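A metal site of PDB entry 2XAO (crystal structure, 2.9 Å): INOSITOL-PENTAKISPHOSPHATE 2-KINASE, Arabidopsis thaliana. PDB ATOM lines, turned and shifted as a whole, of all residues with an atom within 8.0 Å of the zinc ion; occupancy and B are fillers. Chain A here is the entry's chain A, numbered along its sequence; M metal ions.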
ATOM      1  N   GLU A 316       7.583  15.540 -28.795  1.00  0.00           N
ATOM      2  CA  GLU A 316       6.930  14.234 -28.926  1.00  0.00           C
ATOM      3  C   GLU A 316       7.896  13.049 -28.847  1.00  0.00           C
ATOM      4  O   GLU A 316       7.493  11.926 -28.560  1.00  0.00           O
ATOM      5  CB  GLU A 316       6.118  14.170 -30.214  1.00  0.00           C
ATOM      6  CG  GLU A 316       4.759  14.882 -30.133  1.00  0.00           C
ATOM      7  CD  GLU A 316       3.743  14.344 -31.139  1.00  0.00           C
ATOM      8  OE1 GLU A 316       3.411  13.134 -31.095  1.00  0.00           O
ATOM      9  OE2 GLU A 316       3.279  15.134 -31.987  1.00  0.00           O
ATOM     10  N   GLY A 317       9.175  13.311 -29.118  1.00  0.00           N
ATOM     11  CA  GLY A 317      10.228  12.332 -28.895  1.00  0.00           C
ATOM     12  C   GLY A 317      10.790  12.511 -27.499  1.00  0.00           C
ATOM     13  O   GLY A 317      10.713  11.615 -26.662  1.00  0.00           O
ATOM     14  N   ILE A 319      10.028  13.783 -24.736  1.00  0.00           N
ATOM     15  CA  ILE A 319       9.213  13.526 -23.560  1.00  0.00           C
ATOM     16  C   ILE A 319       9.471  12.146 -22.972  1.00  0.00           C
ATOM     17  O   ILE A 319       9.491  11.990 -21.757  1.00  0.00           O
ATOM     18  CB  ILE A 319       7.706  13.734 -23.882  1.00  0.00           C
ATOM     19  CG1 ILE A 319       6.839  13.565 -22.641  1.00  0.00           C
ATOM     20  CG2 ILE A 319       7.225  12.810 -25.020  1.00  0.00           C
ATOM     21  CD1 ILE A 319       6.672  14.831 -21.888  1.00  0.00           C
ATOM     22  N   HIS A 320       9.662  11.139 -23.842  1.00  0.00           N
ATOM     23  CA  HIS A 320       9.928   9.766 -23.391  1.00  0.00           C
ATOM     24  C   HIS A 320      11.239   9.738 -22.604  1.00  0.00           C
ATOM     25  O   HIS A 320      11.316   9.121 -21.527  1.00  0.00           O
ATOM     26  CB  HIS A 320       9.953   8.784 -24.582  1.00  0.00           C
ATOM     27  CG  HIS A 320       8.690   8.749 -25.373  1.00  0.00           C
ATOM     28  ND1 HIS A 320       7.651   7.869 -25.102  1.00  0.00           N
ATOM     29  CD2 HIS A 320       8.270   9.499 -26.423  1.00  0.00           C
ATOM     30  CE1 HIS A 320       6.659   8.093 -25.960  1.00  0.00           C
ATOM     31  NE2 HIS A 320       7.009   9.071 -26.761  1.00  0.00           N
ATOM     32  N   CYS A 321      12.244  10.440 -23.121  1.00  0.00           N
ATOM     33  CA  CYS A 321      13.537  10.502 -22.451  1.00  0.00           C
ATOM     34  C   CYS A 321      13.452  11.186 -21.093  1.00  0.00           C
ATOM     35  O   CYS A 321      14.222  10.872 -20.177  1.00  0.00           O
ATOM     36  CB  CYS A 321      14.553  11.203 -23.323  1.00  0.00           C
ATOM     37  SG  CYS A 321      14.912  10.281 -24.797  1.00  0.00           S
ATOM     38  N   TYR A 323      10.887  11.065 -18.933  1.00  0.00           N
ATOM     39  CA  TYR A 323      10.335  10.148 -17.932  1.00  0.00           C
ATOM     40  C   TYR A 323      11.338   9.127 -17.417  1.00  0.00           C
ATOM     41  O   TYR A 323      11.256   8.683 -16.277  1.00  0.00           O
ATOM     42  CB  TYR A 323       9.068   9.470 -18.437  1.00  0.00           C
ATOM     43  CG  TYR A 323       7.897  10.408 -18.419  1.00  0.00           C
ATOM     44  CD1 TYR A 323       7.240  10.721 -17.217  1.00  0.00           C
ATOM     45  CD2 TYR A 323       7.464  11.015 -19.590  1.00  0.00           C
ATOM     46  CE1 TYR A 323       6.159  11.615 -17.199  1.00  0.00           C
ATOM     47  CE2 TYR A 323       6.381  11.903 -19.586  1.00  0.00           C
ATOM     48  CZ  TYR A 323       5.747  12.191 -18.397  1.00  0.00           C
ATOM     49  OH  TYR A 323       4.691  13.065 -18.434  1.00  0.00           O
ATOM     50  N   ASP A 324      12.300   8.773 -18.274  1.00  0.00           N
ATOM     51  CA  ASP A 324      13.420   7.934 -17.876  1.00  0.00           C
ATOM     52  C   ASP A 324      14.319   8.658 -16.886  1.00  0.00           C
ATOM     53  O   ASP A 324      14.748   8.080 -15.898  1.00  0.00           O
ATOM     54  CB  ASP A 324      14.235   7.504 -19.088  1.00  0.00           C
ATOM     55  CG  ASP A 324      13.481   6.541 -19.963  1.00  0.00           C
ATOM     56  OD1 ASP A 324      12.522   5.946 -19.466  1.00  0.00           O
ATOM     57  OD2 ASP A 324      13.869   6.389 -21.146  1.00  0.00           O
ATOM     58  N   GLN A 328      10.383   7.722 -13.684  1.00  0.00           N
ATOM     59  CA  GLN A 328       8.965   7.384 -13.621  1.00  0.00           C
ATOM     60  C   GLN A 328       8.549   6.535 -14.834  1.00  0.00           C
ATOM     61  O   GLN A 328       9.119   6.677 -15.924  1.00  0.00           O
ATOM     62  CB  GLN A 328       8.107   8.643 -13.536  1.00  0.00           C
ATOM     63  CG  GLN A 328       6.603   8.343 -13.438  1.00  0.00           C
ATOM     64  CD  GLN A 328       5.713   9.530 -13.785  1.00  0.00           C
ATOM     65  OE1 GLN A 328       5.996  10.675 -13.387  1.00  0.00           O
ATOM     66  NE2 GLN A 328       4.626   9.258 -14.518  1.00  0.00           N
ATOM     67  N   PRO A 329       7.555   5.621 -14.651  1.00  0.00           N
ATOM     68  CA  PRO A 329       6.954   4.923 -15.791  1.00  0.00           C
ATOM     69  C   PRO A 329       6.347   5.922 -16.772  1.00  0.00           C
ATOM     70  O   PRO A 329       5.675   6.864 -16.338  1.00  0.00           O
ATOM     71  CB  PRO A 329       5.829   4.101 -15.138  1.00  0.00           C
ATOM     72  CG  PRO A 329       6.216   3.949 -13.717  1.00  0.00           C
ATOM     73  CD  PRO A 329       6.986   5.180 -13.365  1.00  0.00           C
ATOM     74  N   CYS A 330       6.565   5.719 -18.072  1.00  0.00           N
ATOM     75  CA  CYS A 330       6.080   6.642 -19.110  1.00  0.00           C
ATOM     76  C   CYS A 330       4.574   6.517 -19.339  1.00  0.00           C
ATOM     77  O   CYS A 330       4.090   5.464 -19.745  1.00  0.00           O
ATOM     78  CB  CYS A 330       6.828   6.446 -20.446  1.00  0.00           C
ATOM     79  SG  CYS A 330       6.199   7.431 -21.854  1.00  0.00           S
ATOM     80  N   PRO A 331       3.811   7.601 -19.080  1.00  0.00           N
ATOM     81  CA  PRO A 331       2.384   7.654 -19.376  1.00  0.00           C
ATOM     82  C   PRO A 331       2.076   7.911 -20.855  1.00  0.00           C
ATOM     83  O   PRO A 331       0.978   7.612 -21.320  1.00  0.00           O
ATOM     84  CB  PRO A 331       1.892   8.826 -18.518  1.00  0.00           C
ATOM     85  CG  PRO A 331       3.063   9.728 -18.403  1.00  0.00           C
ATOM     86  CD  PRO A 331       4.294   8.864 -18.472  1.00  0.00           C
ATOM     87  N   ILE A 332       3.039   8.473 -21.578  1.00  0.00           N
ATOM     88  CA  ILE A 332       2.829   8.836 -22.969  1.00  0.00           C
ATOM     89  C   ILE A 332       2.688   7.582 -23.806  1.00  0.00           C
ATOM     90  O   ILE A 332       1.782   7.497 -24.639  1.00  0.00           O
ATOM     91  CB  ILE A 332       3.948   9.764 -23.506  1.00  0.00           C
ATOM     92  CG1 ILE A 332       4.284  10.854 -22.473  1.00  0.00           C
ATOM     93  CG2 ILE A 332       3.556  10.361 -24.861  1.00  0.00           C
ATOM     94  CD1 ILE A 332       3.147  11.827 -22.108  1.00  0.00           C
ATOM     95  N   CYS A 333       3.588   6.618 -23.605  1.00  0.00           N
ATOM     96  CA  CYS A 333       3.375   5.250 -24.079  1.00  0.00           C
ATOM     97  C   CYS A 333       2.269   4.651 -23.224  1.00  0.00           C
ATOM     98  O   CYS A 333       2.160   4.975 -22.030  1.00  0.00           O
ATOM     99  CB  CYS A 333       4.647   4.395 -23.914  1.00  0.00           C
ATOM    100  SG  CYS A 333       6.140   5.005 -24.730  1.00  0.00           S
ATOM    101  N   LYS A 334       1.446   3.798 -23.804  1.00  0.00           N
ATOM    102  CA  LYS A 334       0.355   3.196 -23.034  1.00  0.00           C
ATOM    103  C   LYS A 334       0.550   1.698 -22.794  1.00  0.00           C
ATOM    104  O   LYS A 334       1.641   1.167 -22.990  1.00  0.00           O
ATOM    105  CB  LYS A 334      -0.984   3.505 -23.696  1.00  0.00           C
ATOM    106  CG  LYS A 334      -1.452   4.941 -23.523  1.00  0.00           C
ATOM    107  CD  LYS A 334      -2.691   5.164 -24.361  1.00  0.00           C
ATOM    108  CE  LYS A 334      -3.389   6.467 -24.024  1.00  0.00           C
ATOM    109  NZ  LYS A 334      -4.781   6.430 -24.584  1.00  0.00           N
ATOM    110  N   GLU A 342       7.926   4.602 -27.860  1.00  0.00           N
ATOM    111  CA  GLU A 342       8.555   3.590 -28.694  1.00  0.00           C
ATOM    112  C   GLU A 342       9.520   2.756 -27.865  1.00  0.00           C
ATOM    113  O   GLU A 342      10.127   3.272 -26.915  1.00  0.00           O
ATOM    114  CB  GLU A 342       9.309   4.225 -29.865  1.00  0.00           C
ATOM    115  CG  GLU A 342       8.413   4.797 -30.984  1.00  0.00           C
ATOM    116  CD  GLU A 342       7.857   6.182 -30.652  1.00  0.00           C
ATOM    117  OE1 GLU A 342       7.884   6.581 -29.452  1.00  0.00           O
ATOM    118  OE2 GLU A 342       7.388   6.882 -31.576  1.00  0.00           O
ATOM    119  N   LEU A 343       9.663   1.492 -28.231  1.00  0.00           N
ATOM    120  CA  LEU A 343      10.593   0.572 -27.563  1.00  0.00           C
ATOM    121  C   LEU A 343      11.995   0.805 -28.161  1.00  0.00           C
ATOM    122  O   LEU A 343      12.680  -0.141 -28.609  1.00  0.00           O
ATOM    123  CB  LEU A 343      10.106  -0.893 -27.755  1.00  0.00           C
ATOM    124  CG  LEU A 343      10.191  -2.021 -26.691  1.00  0.00           C
ATOM    125  CD1 LEU A 343      11.590  -2.682 -26.596  1.00  0.00           C
ATOM    126  CD2 LEU A 343       9.670  -1.604 -25.294  1.00  0.00           C
ATOM    127  N   LEU A 345      13.534   4.659 -27.790  1.00  0.00           N
ATOM    128  CA  LEU A 345      14.100   5.741 -26.990  1.00  0.00           C
ATOM    129  C   LEU A 345      14.238   5.301 -25.529  1.00  0.00           C
ATOM    130  O   LEU A 345      15.151   5.749 -24.820  1.00  0.00           O
ATOM    131  CB  LEU A 345      13.233   7.014 -27.073  1.00  0.00           C
ATOM    132  CG  LEU A 345      13.114   7.811 -28.376  1.00  0.00           C
ATOM    133  CD1 LEU A 345      12.044   8.863 -28.228  1.00  0.00           C
ATOM    134  CD2 LEU A 345      14.432   8.436 -28.810  1.00  0.00           C
ATOM    135  N   HIS A 346      13.325   4.445 -25.089  1.00  0.00           N
ATOM    136  CA  HIS A 346      13.363   3.887 -23.742  1.00  0.00           C
ATOM    137  C   HIS A 346      14.470   2.828 -23.641  1.00  0.00           C
ATOM    138  O   HIS A 346      14.771   2.345 -22.549  1.00  0.00           O
ATOM    139  CB  HIS A 346      11.996   3.287 -23.362  1.00  0.00           C
ATOM    140  CG  HIS A 346      10.914   4.303 -23.143  1.00  0.00           C
ATOM    141  ND1 HIS A 346      10.893   5.146 -22.045  1.00  0.00           N
ATOM    142  CD2 HIS A 346       9.818   4.614 -23.872  1.00  0.00           C
ATOM    143  CE1 HIS A 346       9.833   5.932 -22.128  1.00  0.00           C
ATOM    144  NE2 HIS A 346       9.159   5.630 -23.224  1.00  0.00           N
HETATM  145 ZN    ZN M   1       7.377   6.412 -23.510  1.00  0.00          ZN
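The side-chain carboxylate (OD1) of Asp 324 is in hydrogen-bond range of a ring nitrogen (ND1) of His 346 (3.2 Å). NE2 of His 320 lies close to O of Glu 316, at 3.4 Å. The side-chain sulfur (SG) of Cys 333 lies close to the backbone NH (N) of Glu 342 (3.6 Å). The side-chain sulfur of Cys 330 sits close to the backbone NH of Ile 332.
Within 4 Å of the zinc ion: His 320, Cys 330, Cys 333 and His 346. The nearest printed residue that does not touch the zinc ion is Glu 342 (4.7 Å).
The zinc ion is bound by a ring nitrogen (NE2) of His 346 (2.0 Å), a ring nitrogen (ND1) of His 320 (2.2 Å), the side-chain sulfur (SG) of Cys 333 (2.2 Å) and the side-chain sulfur (SG) of Cys 330 (2.3 Å). The zinc ion has four donor atoms within binding distance.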
